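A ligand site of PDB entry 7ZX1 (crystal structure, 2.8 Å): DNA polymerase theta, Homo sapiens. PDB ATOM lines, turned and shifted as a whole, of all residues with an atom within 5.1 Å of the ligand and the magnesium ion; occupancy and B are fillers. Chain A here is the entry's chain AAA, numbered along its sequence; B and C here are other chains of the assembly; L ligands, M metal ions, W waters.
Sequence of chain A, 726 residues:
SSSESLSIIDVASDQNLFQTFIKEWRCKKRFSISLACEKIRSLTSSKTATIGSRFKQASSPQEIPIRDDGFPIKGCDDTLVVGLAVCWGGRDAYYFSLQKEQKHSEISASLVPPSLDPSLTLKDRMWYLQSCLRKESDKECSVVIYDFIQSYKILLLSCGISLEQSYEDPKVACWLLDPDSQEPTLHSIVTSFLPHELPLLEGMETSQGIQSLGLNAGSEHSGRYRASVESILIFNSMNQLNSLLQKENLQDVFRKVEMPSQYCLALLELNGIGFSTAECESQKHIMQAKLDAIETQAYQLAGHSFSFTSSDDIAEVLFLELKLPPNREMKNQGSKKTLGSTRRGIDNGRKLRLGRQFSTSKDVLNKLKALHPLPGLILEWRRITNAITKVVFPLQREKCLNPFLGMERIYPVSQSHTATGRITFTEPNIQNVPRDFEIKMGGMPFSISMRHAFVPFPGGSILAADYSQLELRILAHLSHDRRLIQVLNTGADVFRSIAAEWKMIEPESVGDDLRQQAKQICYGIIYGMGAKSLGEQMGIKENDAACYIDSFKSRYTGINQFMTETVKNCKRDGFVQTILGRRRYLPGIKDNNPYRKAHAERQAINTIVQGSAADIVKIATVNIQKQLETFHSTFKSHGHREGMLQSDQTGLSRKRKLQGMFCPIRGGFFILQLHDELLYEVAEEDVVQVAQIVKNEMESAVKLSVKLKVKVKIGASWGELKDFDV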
ATOM      1  N   ARG A 422     -25.074 -22.482  25.754  1.00  0.00           N
ATOM      2  CA  ARG A 422     -24.935 -22.307  24.287  1.00  0.00           C
ATOM      3  C   ARG A 422     -26.233 -22.733  23.609  1.00  0.00           C
ATOM      4  O   ARG A 422     -26.971 -23.567  24.163  1.00  0.00           O
ATOM      5  CB  ARG A 422     -23.764 -23.151  23.762  1.00  0.00           C
ATOM      6  CG  ARG A 422     -22.404 -22.571  24.096  1.00  0.00           C
ATOM      7  CD  ARG A 422     -21.294 -23.195  23.273  1.00  0.00           C
ATOM      8  NE  ARG A 422     -20.100 -22.356  23.243  1.00  0.00           N
ATOM      9  CZ  ARG A 422     -19.074 -22.574  22.439  1.00  0.00           C
ATOM     10  NH1 ARG A 422     -19.101 -23.590  21.601  1.00  0.00           N
ATOM     11  NH2 ARG A 422     -18.018 -21.790  22.494  1.00  0.00           N
ATOM     12  N   ASP A 466     -19.394 -10.602  15.264  1.00  0.00           N
ATOM     13  CA  ASP A 466     -18.685 -11.552  16.157  1.00  0.00           C
ATOM     14  C   ASP A 466     -17.991 -10.751  17.269  1.00  0.00           C
ATOM     15  O   ASP A 466     -17.416  -9.665  17.049  1.00  0.00           O
ATOM     16  CB  ASP A 466     -17.694 -12.386  15.305  1.00  0.00           C
ATOM     17  CG  ASP A 466     -16.309 -11.812  15.075  1.00  0.00           C
ATOM     18  OD1 ASP A 466     -15.409 -12.188  15.862  1.00  0.00           O
ATOM     19  OD2 ASP A 466     -16.138 -11.034  14.090  1.00  0.00           O
ATOM     20  N   TYR A 467     -18.070 -11.250  18.478  1.00  0.00           N
ATOM     21  CA  TYR A 467     -17.307 -10.722  19.631  1.00  0.00           C
ATOM     22  C   TYR A 467     -15.849 -11.126  19.474  1.00  0.00           C
ATOM     23  O   TYR A 467     -15.546 -12.265  19.163  1.00  0.00           O
ATOM     24  CB  TYR A 467     -17.803 -11.354  20.934  1.00  0.00           C
ATOM     25  CG  TYR A 467     -19.063 -10.736  21.485  1.00  0.00           C
ATOM     26  CD1 TYR A 467     -19.059  -9.422  21.908  1.00  0.00           C
ATOM     27  CD2 TYR A 467     -20.249 -11.464  21.602  1.00  0.00           C
ATOM     28  CE1 TYR A 467     -20.201  -8.821  22.363  1.00  0.00           C
ATOM     29  CE2 TYR A 467     -21.396 -10.876  22.106  1.00  0.00           C
ATOM     30  CZ  TYR A 467     -21.372  -9.543  22.467  1.00  0.00           C
ATOM     31  OH  TYR A 467     -22.475  -8.916  22.962  1.00  0.00           O
ATOM     32  N   SER A 468     -14.959 -10.196  19.641  1.00  0.00           N
ATOM     33  CA  SER A 468     -13.483 -10.473  19.659  1.00  0.00           C
ATOM     34  C   SER A 468     -13.041 -11.093  20.989  1.00  0.00           C
ATOM     35  O   SER A 468     -13.117 -10.414  21.952  1.00  0.00           O
ATOM     36  CB  SER A 468     -12.790  -9.191  19.309  1.00  0.00           C
ATOM     37  OG  SER A 468     -13.355  -8.662  18.102  1.00  0.00           O
ATOM     38  N   GLN A 469     -12.705 -12.379  21.014  1.00  0.00           N
ATOM     39  CA  GLN A 469     -12.121 -13.057  22.194  1.00  0.00           C
ATOM     40  C   GLN A 469     -13.024 -12.804  23.410  1.00  0.00           C
ATOM     41  O   GLN A 469     -12.535 -12.331  24.454  1.00  0.00           O
ATOM     42  CB  GLN A 469     -10.709 -12.555  22.518  1.00  0.00           C
ATOM     43  CG  GLN A 469      -9.680 -12.829  21.436  1.00  0.00           C
ATOM     44  CD  GLN A 469      -9.528 -11.649  20.513  1.00  0.00           C
ATOM     45  OE1 GLN A 469      -9.344 -10.512  20.948  1.00  0.00           O
ATOM     46  NE2 GLN A 469      -9.568 -11.930  19.218  1.00  0.00           N
ATOM     47  N   GLU A 471     -14.547 -14.977  25.440  1.00  0.00           N
ATOM     48  CA  GLU A 471     -14.188 -15.853  26.592  1.00  0.00           C
ATOM     49  C   GLU A 471     -12.927 -15.313  27.263  1.00  0.00           C
ATOM     50  O   GLU A 471     -12.853 -15.401  28.507  1.00  0.00           O
ATOM     51  CB  GLU A 471     -14.095 -17.337  26.174  1.00  0.00           C
ATOM     52  CG  GLU A 471     -15.401 -18.080  26.367  1.00  0.00           C
ATOM     53  CD  GLU A 471     -15.563 -19.490  25.781  1.00  0.00           C
ATOM     54  OE1 GLU A 471     -14.892 -20.433  26.254  1.00  0.00           O
ATOM     55  OE2 GLU A 471     -16.403 -19.650  24.870  1.00  0.00           O
ATOM     56  N   ASP A 493      -2.829 -10.267  17.161  1.00  0.00           N
ATOM     57  CA  ASP A 493      -3.613 -11.536  17.283  1.00  0.00           C
ATOM     58  C   ASP A 493      -2.818 -12.551  18.140  1.00  0.00           C
ATOM     59  O   ASP A 493      -1.695 -12.938  17.713  1.00  0.00           O
ATOM     60  CB  ASP A 493      -4.025 -12.132  15.944  1.00  0.00           C
ATOM     61  CG  ASP A 493      -5.151 -13.143  16.087  1.00  0.00           C
ATOM     62  OD1 ASP A 493      -6.165 -12.862  16.770  1.00  0.00           O
ATOM     63  OD2 ASP A 493      -5.019 -14.238  15.537  1.00  0.00           O
ATOM     64  N   PHE A 495      -3.336 -15.677  18.773  1.00  0.00           N
ATOM     65  CA  PHE A 495      -3.164 -16.993  18.072  1.00  0.00           C
ATOM     66  C   PHE A 495      -1.965 -16.908  17.111  1.00  0.00           C
ATOM     67  O   PHE A 495      -1.131 -17.827  17.117  1.00  0.00           O
ATOM     68  CB  PHE A 495      -4.493 -17.450  17.469  1.00  0.00           C
ATOM     69  CG  PHE A 495      -5.653 -17.376  18.445  1.00  0.00           C
ATOM     70  CD1 PHE A 495      -5.548 -17.940  19.703  1.00  0.00           C
ATOM     71  CD2 PHE A 495      -6.829 -16.733  18.136  1.00  0.00           C
ATOM     72  CE1 PHE A 495      -6.578 -17.855  20.624  1.00  0.00           C
ATOM     73  CE2 PHE A 495      -7.871 -16.646  19.050  1.00  0.00           C
ATOM     74  CZ  PHE A 495      -7.732 -17.199  20.295  1.00  0.00           C
ATOM     75  N   ARG A 515      -3.405 -21.161  12.304  1.00  0.00           N
ATOM     76  CA  ARG A 515      -3.983 -20.217  13.309  1.00  0.00           C
ATOM     77  C   ARG A 515      -5.020 -20.953  14.182  1.00  0.00           C
ATOM     78  O   ARG A 515      -5.033 -20.728  15.397  1.00  0.00           O
ATOM     79  CB  ARG A 515      -4.625 -18.990  12.668  1.00  0.00           C
ATOM     80  CG  ARG A 515      -5.036 -17.935  13.682  1.00  0.00           C
ATOM     81  CD  ARG A 515      -5.469 -16.655  13.020  1.00  0.00           C
ATOM     82  NE  ARG A 515      -6.096 -15.765  13.982  1.00  0.00           N
ATOM     83  CZ  ARG A 515      -7.354 -15.834  14.388  1.00  0.00           C
ATOM     84  NH1 ARG A 515      -7.818 -14.956  15.264  1.00  0.00           N
ATOM     85  NH2 ARG A 515      -8.145 -16.795  13.925  1.00  0.00           N
ATOM     86  N   GLN A 516      -5.807 -21.841  13.572  1.00  0.00           N
ATOM     87  CA  GLN A 516      -6.762 -22.756  14.256  1.00  0.00           C
ATOM     88  C   GLN A 516      -5.986 -23.694  15.194  1.00  0.00           C
ATOM     89  O   GLN A 516      -6.446 -23.875  16.345  1.00  0.00           O
ATOM     90  CB  GLN A 516      -7.588 -23.526  13.227  1.00  0.00           C
ATOM     91  CG  GLN A 516      -8.443 -22.617  12.363  1.00  0.00           C
ATOM     92  CD  GLN A 516      -9.569 -21.975  13.146  1.00  0.00           C
ATOM     93  OE1 GLN A 516      -9.467 -20.853  13.649  1.00  0.00           O
ATOM     94  NE2 GLN A 516     -10.645 -22.709  13.255  1.00  0.00           N
ATOM     95  N   LYS A 519      -5.066 -21.581  18.135  1.00  0.00           N
ATOM     96  CA  LYS A 519      -6.320 -21.284  18.856  1.00  0.00           C
ATOM     97  C   LYS A 519      -6.607 -22.460  19.814  1.00  0.00           C
ATOM     98  O   LYS A 519      -6.834 -22.196  21.013  1.00  0.00           O
ATOM     99  CB  LYS A 519      -7.465 -21.075  17.867  1.00  0.00           C
ATOM    100  CG  LYS A 519      -8.826 -20.787  18.486  1.00  0.00           C
ATOM    101  CD  LYS A 519      -9.874 -20.451  17.457  1.00  0.00           C
ATOM    102  CE  LYS A 519      -9.694 -19.060  16.899  1.00  0.00           C
ATOM    103  NZ  LYS A 519     -10.694 -18.757  15.837  1.00  0.00           N
ATOM    104  N   GLN A 520      -6.520 -23.699  19.310  1.00  0.00           N
ATOM    105  CA  GLN A 520      -6.763 -24.956  20.071  1.00  0.00           C
ATOM    106  C   GLN A 520      -5.760 -25.027  21.229  1.00  0.00           C
ATOM    107  O   GLN A 520      -6.155 -25.395  22.347  1.00  0.00           O
ATOM    108  CB  GLN A 520      -6.535 -26.192  19.189  1.00  0.00           C
ATOM    109  CG  GLN A 520      -7.758 -26.939  18.732  1.00  0.00           C
ATOM    110  CD  GLN A 520      -7.405 -28.393  18.484  1.00  0.00           C
ATOM    111  OE1 GLN A 520      -7.566 -29.254  19.344  1.00  0.00           O
ATOM    112  NE2 GLN A 520      -6.984 -28.700  17.252  1.00  0.00           N
ATOM    113  N   TYR A 523      -6.679 -21.969  24.050  1.00  0.00           N
ATOM    114  CA  TYR A 523      -7.900 -22.316  24.853  1.00  0.00           C
ATOM    115  C   TYR A 523      -7.656 -23.636  25.594  1.00  0.00           C
ATOM    116  O   TYR A 523      -8.071 -23.746  26.755  1.00  0.00           O
ATOM    117  CB  TYR A 523      -9.146 -22.298  23.980  1.00  0.00           C
ATOM    118  CG  TYR A 523      -9.576 -20.916  23.554  1.00  0.00           C
ATOM    119  CD1 TYR A 523      -9.925 -19.965  24.489  1.00  0.00           C
ATOM    120  CD2 TYR A 523      -9.692 -20.578  22.215  1.00  0.00           C
ATOM    121  CE1 TYR A 523     -10.333 -18.690  24.113  1.00  0.00           C
ATOM    122  CE2 TYR A 523     -10.096 -19.312  21.816  1.00  0.00           C
ATOM    123  CZ  TYR A 523     -10.404 -18.360  22.766  1.00  0.00           C
ATOM    124  OH  TYR A 523     -10.818 -17.109  22.393  1.00  0.00           O
ATOM    125  N   GLY A 524      -6.983 -24.590  24.952  1.00  0.00           N
ATOM    126  CA  GLY A 524      -6.621 -25.888  25.561  1.00  0.00           C
ATOM    127  C   GLY A 524      -5.871 -25.700  26.867  1.00  0.00           C
ATOM    128  O   GLY A 524      -6.327 -26.203  27.932  1.00  0.00           O
ATOM    129  N   TYR A 527      -7.912 -24.090  29.656  1.00  0.00           N
ATOM    130  CA  TYR A 527      -9.016 -24.904  30.226  1.00  0.00           C
ATOM    131  C   TYR A 527      -8.489 -26.253  30.707  1.00  0.00           C
ATOM    132  O   TYR A 527      -9.310 -27.200  30.845  1.00  0.00           O
ATOM    133  CB  TYR A 527     -10.192 -24.990  29.231  1.00  0.00           C
ATOM    134  CG  TYR A 527     -10.908 -23.684  28.986  1.00  0.00           C
ATOM    135  CD1 TYR A 527     -11.502 -22.989  30.028  1.00  0.00           C
ATOM    136  CD2 TYR A 527     -11.010 -23.130  27.720  1.00  0.00           C
ATOM    137  CE1 TYR A 527     -12.167 -21.786  29.826  1.00  0.00           C
ATOM    138  CE2 TYR A 527     -11.679 -21.930  27.496  1.00  0.00           C
ATOM    139  CZ  TYR A 527     -12.270 -21.249  28.558  1.00  0.00           C
ATOM    140  OH  TYR A 527     -12.924 -20.065  28.361  1.00  0.00           O
ATOM    141  N   ASN A 606     -14.392 -23.900  33.032  1.00  0.00           N
ATOM    142  CA  ASN A 606     -14.861 -23.645  31.645  1.00  0.00           C
ATOM    143  C   ASN A 606     -16.344 -23.220  31.662  1.00  0.00           C
ATOM    144  O   ASN A 606     -16.727 -22.369  30.834  1.00  0.00           O
ATOM    145  CB  ASN A 606     -14.653 -24.875  30.771  1.00  0.00           C
ATOM    146  CG  ASN A 606     -15.260 -24.747  29.394  1.00  0.00           C
ATOM    147  OD1 ASN A 606     -16.230 -25.438  29.096  1.00  0.00           O
ATOM    148  ND2 ASN A 606     -14.706 -23.880  28.566  1.00  0.00           N
ATOM    149  N   GLN A 610     -17.452 -19.960  29.570  1.00  0.00           N
ATOM    150  CA  GLN A 610     -18.213 -20.315  28.341  1.00  0.00           C
ATOM    151  C   GLN A 610     -19.702 -20.010  28.598  1.00  0.00           C
ATOM    152  O   GLN A 610     -20.351 -19.481  27.683  1.00  0.00           O
ATOM    153  CB  GLN A 610     -18.013 -21.783  27.969  1.00  0.00           C
ATOM    154  CG  GLN A 610     -18.654 -22.187  26.662  1.00  0.00           C
ATOM    155  CD  GLN A 610     -18.395 -23.631  26.294  1.00  0.00           C
ATOM    156  OE1 GLN A 610     -19.299 -24.466  26.247  1.00  0.00           O
ATOM    157  NE2 GLN A 610     -17.144 -23.942  26.021  1.00  0.00           N
ATOM    158  N   ASP A 676     -20.416 -17.048  19.480  1.00  0.00           N
ATOM    159  CA  ASP A 676     -19.954 -15.661  19.793  1.00  0.00           C
ATOM    160  C   ASP A 676     -20.291 -14.753  18.610  1.00  0.00           C
ATOM    161  O   ASP A 676     -19.727 -13.653  18.542  1.00  0.00           O
ATOM    162  CB  ASP A 676     -18.461 -15.618  20.105  1.00  0.00           C
ATOM    163  CG  ASP A 676     -17.568 -15.769  18.874  1.00  0.00           C
ATOM    164  OD1 ASP A 676     -18.007 -16.428  17.883  1.00  0.00           O
ATOM    165  OD2 ASP A 676     -16.444 -15.202  18.899  1.00  0.00           O
ATOM    166  P    DC B   3      -6.121 -33.525  28.264  1.00  0.00           P
ATOM    167  OP1  DC B   3      -6.448 -34.331  27.010  1.00  0.00           O
ATOM    168  OP2  DC B   3      -4.650 -33.175  28.475  1.00  0.00           O
ATOM    169  O5'  DC B   3      -6.878 -32.093  28.136  1.00  0.00           O
ATOM    170  C5'  DC B   3      -8.304 -32.050  27.929  1.00  0.00           C
ATOM    171  C4'  DC B   3      -8.781 -30.696  28.370  1.00  0.00           C
ATOM    172  O4'  DC B   3      -8.158 -29.712  27.550  1.00  0.00           O
ATOM    173  C3'  DC B   3     -10.275 -30.447  28.276  1.00  0.00           C
ATOM    174  O3'  DC B   3     -10.881 -30.744  29.525  1.00  0.00           O
ATOM    175  C2'  DC B   3     -10.354 -28.954  28.024  1.00  0.00           C
ATOM    176  C1'  DC B   3      -9.044 -28.635  27.302  1.00  0.00           C
ATOM    177  N1   DC B   3      -9.156 -28.485  25.837  1.00  0.00           N
ATOM    178  C2   DC B   3      -9.799 -27.358  25.333  1.00  0.00           C
ATOM    179  O2   DC B   3     -10.279 -26.537  26.121  1.00  0.00           O
ATOM    180  N3   DC B   3      -9.885 -27.193  23.999  1.00  0.00           N
ATOM    181  C4   DC B   3      -9.373 -28.098  23.163  1.00  0.00           C
ATOM    182  N4   DC B   3      -9.483 -27.856  21.876  1.00  0.00           N
ATOM    183  C5   DC B   3      -8.721 -29.276  23.654  1.00  0.00           C
ATOM    184  C6   DC B   3      -8.642 -29.418  24.991  1.00  0.00           C
ATOM    185  P    DC B   4     -12.116 -31.758  29.410  1.00  0.00           P
ATOM    186  OP1  DC B   4     -12.520 -32.300  30.775  1.00  0.00           O
ATOM    187  OP2  DC B   4     -11.917 -32.796  28.326  1.00  0.00           O
ATOM    188  O5'  DC B   4     -13.245 -30.685  28.967  1.00  0.00           O
ATOM    189  C5'  DC B   4     -13.680 -29.755  29.963  1.00  0.00           C
ATOM    190  C4'  DC B   4     -14.571 -28.727  29.308  1.00  0.00           C
ATOM    191  O4'  DC B   4     -13.806 -28.069  28.288  1.00  0.00           O
ATOM    192  C3'  DC B   4     -15.823 -29.252  28.610  1.00  0.00           C
ATOM    193  O3'  DC B   4     -16.937 -29.205  29.512  1.00  0.00           O
ATOM    194  C2'  DC B   4     -16.048 -28.203  27.540  1.00  0.00           C
ATOM    195  C1'  DC B   4     -14.684 -27.574  27.303  1.00  0.00           C
ATOM    196  N1   DC B   4     -14.130 -27.912  25.974  1.00  0.00           N
ATOM    197  C2   DC B   4     -14.459 -27.074  24.917  1.00  0.00           C
ATOM    198  O2   DC B   4     -15.172 -26.087  25.164  1.00  0.00           O
ATOM    199  N3   DC B   4     -13.990 -27.338  23.684  1.00  0.00           N
ATOM    200  C4   DC B   4     -13.229 -28.414  23.475  1.00  0.00           C
ATOM    201  N4   DC B   4     -12.798 -28.630  22.249  1.00  0.00           N
ATOM    202  C5   DC B   4     -12.883 -29.296  24.548  1.00  0.00           C
ATOM    203  C6   DC B   4     -13.359 -29.025  25.768  1.00  0.00           C
ATOM    204  P   DDG C  13     -15.793 -22.462  13.125  1.00  0.00           P
ATOM    205  OP1 DDG C  13     -16.030 -21.235  12.293  1.00  0.00           O
ATOM    206  OP2 DDG C  13     -14.425 -23.033  13.374  1.00  0.00           O
ATOM    207  O5' DDG C  13     -16.457 -22.330  14.597  1.00  0.00           O
ATOM    208  C5' DDG C  13     -17.499 -21.428  14.809  1.00  0.00           C
ATOM    209  C4' DDG C  13     -17.893 -21.488  16.276  1.00  0.00           C
ATOM    210  O4' DDG C  13     -17.825 -22.788  16.784  1.00  0.00           O
ATOM    211  C3' DDG C  13     -16.938 -20.678  17.119  1.00  0.00           C
ATOM    212  C2' DDG C  13     -16.794 -21.409  18.426  1.00  0.00           C
ATOM    213  C1' DDG C  13     -17.376 -22.776  18.143  1.00  0.00           C
ATOM    214  N9  DDG C  13     -16.329 -23.816  18.305  1.00  0.00           N
ATOM    215  C8  DDG C  13     -15.589 -24.340  17.351  1.00  0.00           C
ATOM    216  N7  DDG C  13     -14.781 -25.311  17.878  1.00  0.00           N
ATOM    217  C5  DDG C  13     -15.025 -25.384  19.166  1.00  0.00           C
ATOM    218  C6  DDG C  13     -14.500 -26.161  20.282  1.00  0.00           C
ATOM    219  O6  DDG C  13     -13.632 -27.045  20.107  1.00  0.00           O
ATOM    220  N1  DDG C  13     -15.012 -25.933  21.496  1.00  0.00           N
ATOM    221  C2  DDG C  13     -15.964 -25.029  21.694  1.00  0.00           C
ATOM    222  N2  DDG C  13     -16.432 -24.878  22.941  1.00  0.00           N
ATOM    223  N3  DDG C  13     -16.497 -24.264  20.705  1.00  0.00           N
ATOM    224  C4  DDG C  13     -16.045 -24.400  19.446  1.00  0.00           C
HETATM  225  P1  LIG L   1     -11.531 -15.503  16.130  1.00  0.00           P
HETATM  226  O1  LIG L   1     -11.145 -16.236  14.868  1.00  0.00           O
HETATM  227  O2  LIG L   1     -13.023 -15.176  16.183  1.00  0.00           O
HETATM  228  O3  LIG L   1     -10.655 -14.297  16.377  1.00  0.00           O
HETATM  229  O4  LIG L   1     -11.219 -16.423  17.411  1.00  0.00           O
HETATM  230  P2  LIG L   1     -12.000 -16.523  18.800  1.00  0.00           P
HETATM  231  O5  LIG L   1     -11.110 -16.643  19.987  1.00  0.00           O
HETATM  232  O6  LIG L   1     -13.194 -15.614  18.863  1.00  0.00           O
HETATM  233  O7  LIG L   1     -12.516 -18.002  18.546  1.00  0.00           O
HETATM  234  P3  LIG L   1     -13.742 -18.578  17.734  1.00  0.00           P
HETATM  235  O8  LIG L   1     -13.172 -19.644  16.855  1.00  0.00           O
HETATM  236  O9  LIG L   1     -14.573 -17.443  17.215  1.00  0.00           O
HETATM  237  O10 LIG L   1     -14.463 -19.321  18.971  1.00  0.00           O
HETATM  238  C1  LIG L   1     -15.301 -18.610  19.886  1.00  0.00           C
HETATM  239  C2  LIG L   1     -15.096 -19.164  21.274  1.00  0.00           C
HETATM  240  O11 LIG L   1     -15.378 -20.586  21.342  1.00  0.00           O
HETATM  241  C3  LIG L   1     -13.683 -19.041  21.803  1.00  0.00           C
HETATM  242  C4  LIG L   1     -13.663 -20.092  22.901  1.00  0.00           C
HETATM  243  C5  LIG L   1     -14.496 -21.199  22.289  1.00  0.00           C
HETATM  244  N1  LIG L   1     -13.635 -22.152  21.605  1.00  0.00           N
HETATM  245  C6  LIG L   1     -13.233 -22.167  20.292  1.00  0.00           C
HETATM  246  N2  LIG L   1     -12.414 -23.161  20.002  1.00  0.00           N
HETATM  247  C7  LIG L   1     -12.231 -23.786  21.237  1.00  0.00           C
HETATM  248  C8  LIG L   1     -11.419 -24.889  21.582  1.00  0.00           C
HETATM  249  O12 LIG L   1     -10.667 -25.556  20.858  1.00  0.00           O
HETATM  250  N3  LIG L   1     -11.500 -25.169  22.935  1.00  0.00           N
HETATM  251  C9  LIG L   1     -12.281 -24.515  23.849  1.00  0.00           C
HETATM  252  N4  LIG L   1     -12.203 -24.984  25.106  1.00  0.00           N
HETATM  253  N5  LIG L   1     -13.073 -23.487  23.537  1.00  0.00           N
HETATM  254  C10 LIG L   1     -12.985 -23.172  22.225  1.00  0.00           C
HETATM  255 MG    MG M   1     -14.674 -15.367  17.449  1.00  0.00          MG
HETATM  256  O   HOH W   1     -16.283 -15.280  15.906  1.00  0.00           O
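O of Asp 676 lies within hydrogen-bond range of N of Tyr 467 (2.9 Å). The side-chain amide oxygen (OE1) of Gln 520 sits close to N4 of DC 3 of chain B (3.5 Å). The side-chain amino group (NZ) of Lys 519 lies within hydrogen-bond range of the side-chain amide oxygen (OE1) of Gln 516. O2 of DC 4 of chain B lies within hydrogen-bond range of the side-chain amide nitrogen of Gln 610 (3.0 Å). OD2 of Asp 493 is in salt-bridge range of NE of Arg 515 (2.4 Å). The guanidinium group (NH1) of Arg 422 is in hydrogen-bond range of N3 of DDG 13 of chain C (2.8 Å). N2 of DDG 13 of chain C is in hydrogen-bond range of NE2 of Gln 610 (3.3 Å). The side-chain hydroxyl (OH) of Tyr 527 is in hydrogen-bond range of the side-chain carboxylate (OE1) of Glu 471 (2.9 Å).
The magnesium ion is bound by an oxygen (O6) of the ligand (2.1 Å), an oxygen (O2) of the ligand (2.1 Å), an oxygen (O9) of the ligand (2.1 Å), water W1 (2.2 Å) and the side-chain carboxylate of Asp 676 (2.3 Å).
Asp 466 touches the magnesium ion (OD1 to MG, 3.6 Å). Tyr 467 touches the magnesium ion. Three residues have an atom within 4 Å of the magnesium ion: Asp 466, Tyr 467 and Asp 676.
Water W1 lies within hydrogen-bond range of OD1 of Asp 676 (2.9 Å) and OD1 of Asp 466 (3.2 Å).
O6 of DDG 13 of chain C sits close to O12 of the ligand, 3.4 Å away. Merely in contact with the ligand: Phe 495 (3.4 Å), Glu 471 (3.4 Å), Tyr 527 (3.4 Å), Asp 466 (3.8 Å), Gln 469 (3.9 Å) and Gln 520 (3.9 Å). Hydrophobic or aromatic side chains within 4 Å of the ligand: Phe 495, Tyr 523 and Tyr 527. Of the 21 residues printed, 14 come within 4 Å of the ligand. The nearest printed residue that does not touch the ligand is Tyr 467 (4.1 Å).
The side-chain hydroxyl of Tyr 523 lies within hydrogen-bond range of an oxygen (O5) of the ligand (2.5 Å). A nitrogen (N4) of the ligand lies within hydrogen-bond range of O2 of DC 3 of chain B (2.7 Å). O1 of the ligand lies within salt-bridge range of NZ of Lys 519, at 2.7 Å. O2 of DC 4 of chain B lies close to a nitrogen (N4) of the ligand. The guanidinium group (NH1) of Arg 515 lies within salt-bridge range of an oxygen (O3) of the ligand (3.1 Å). NH2 of Arg 422 sits at hydrogen-bond distance from O11 of the ligand, at 3.1 Å.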
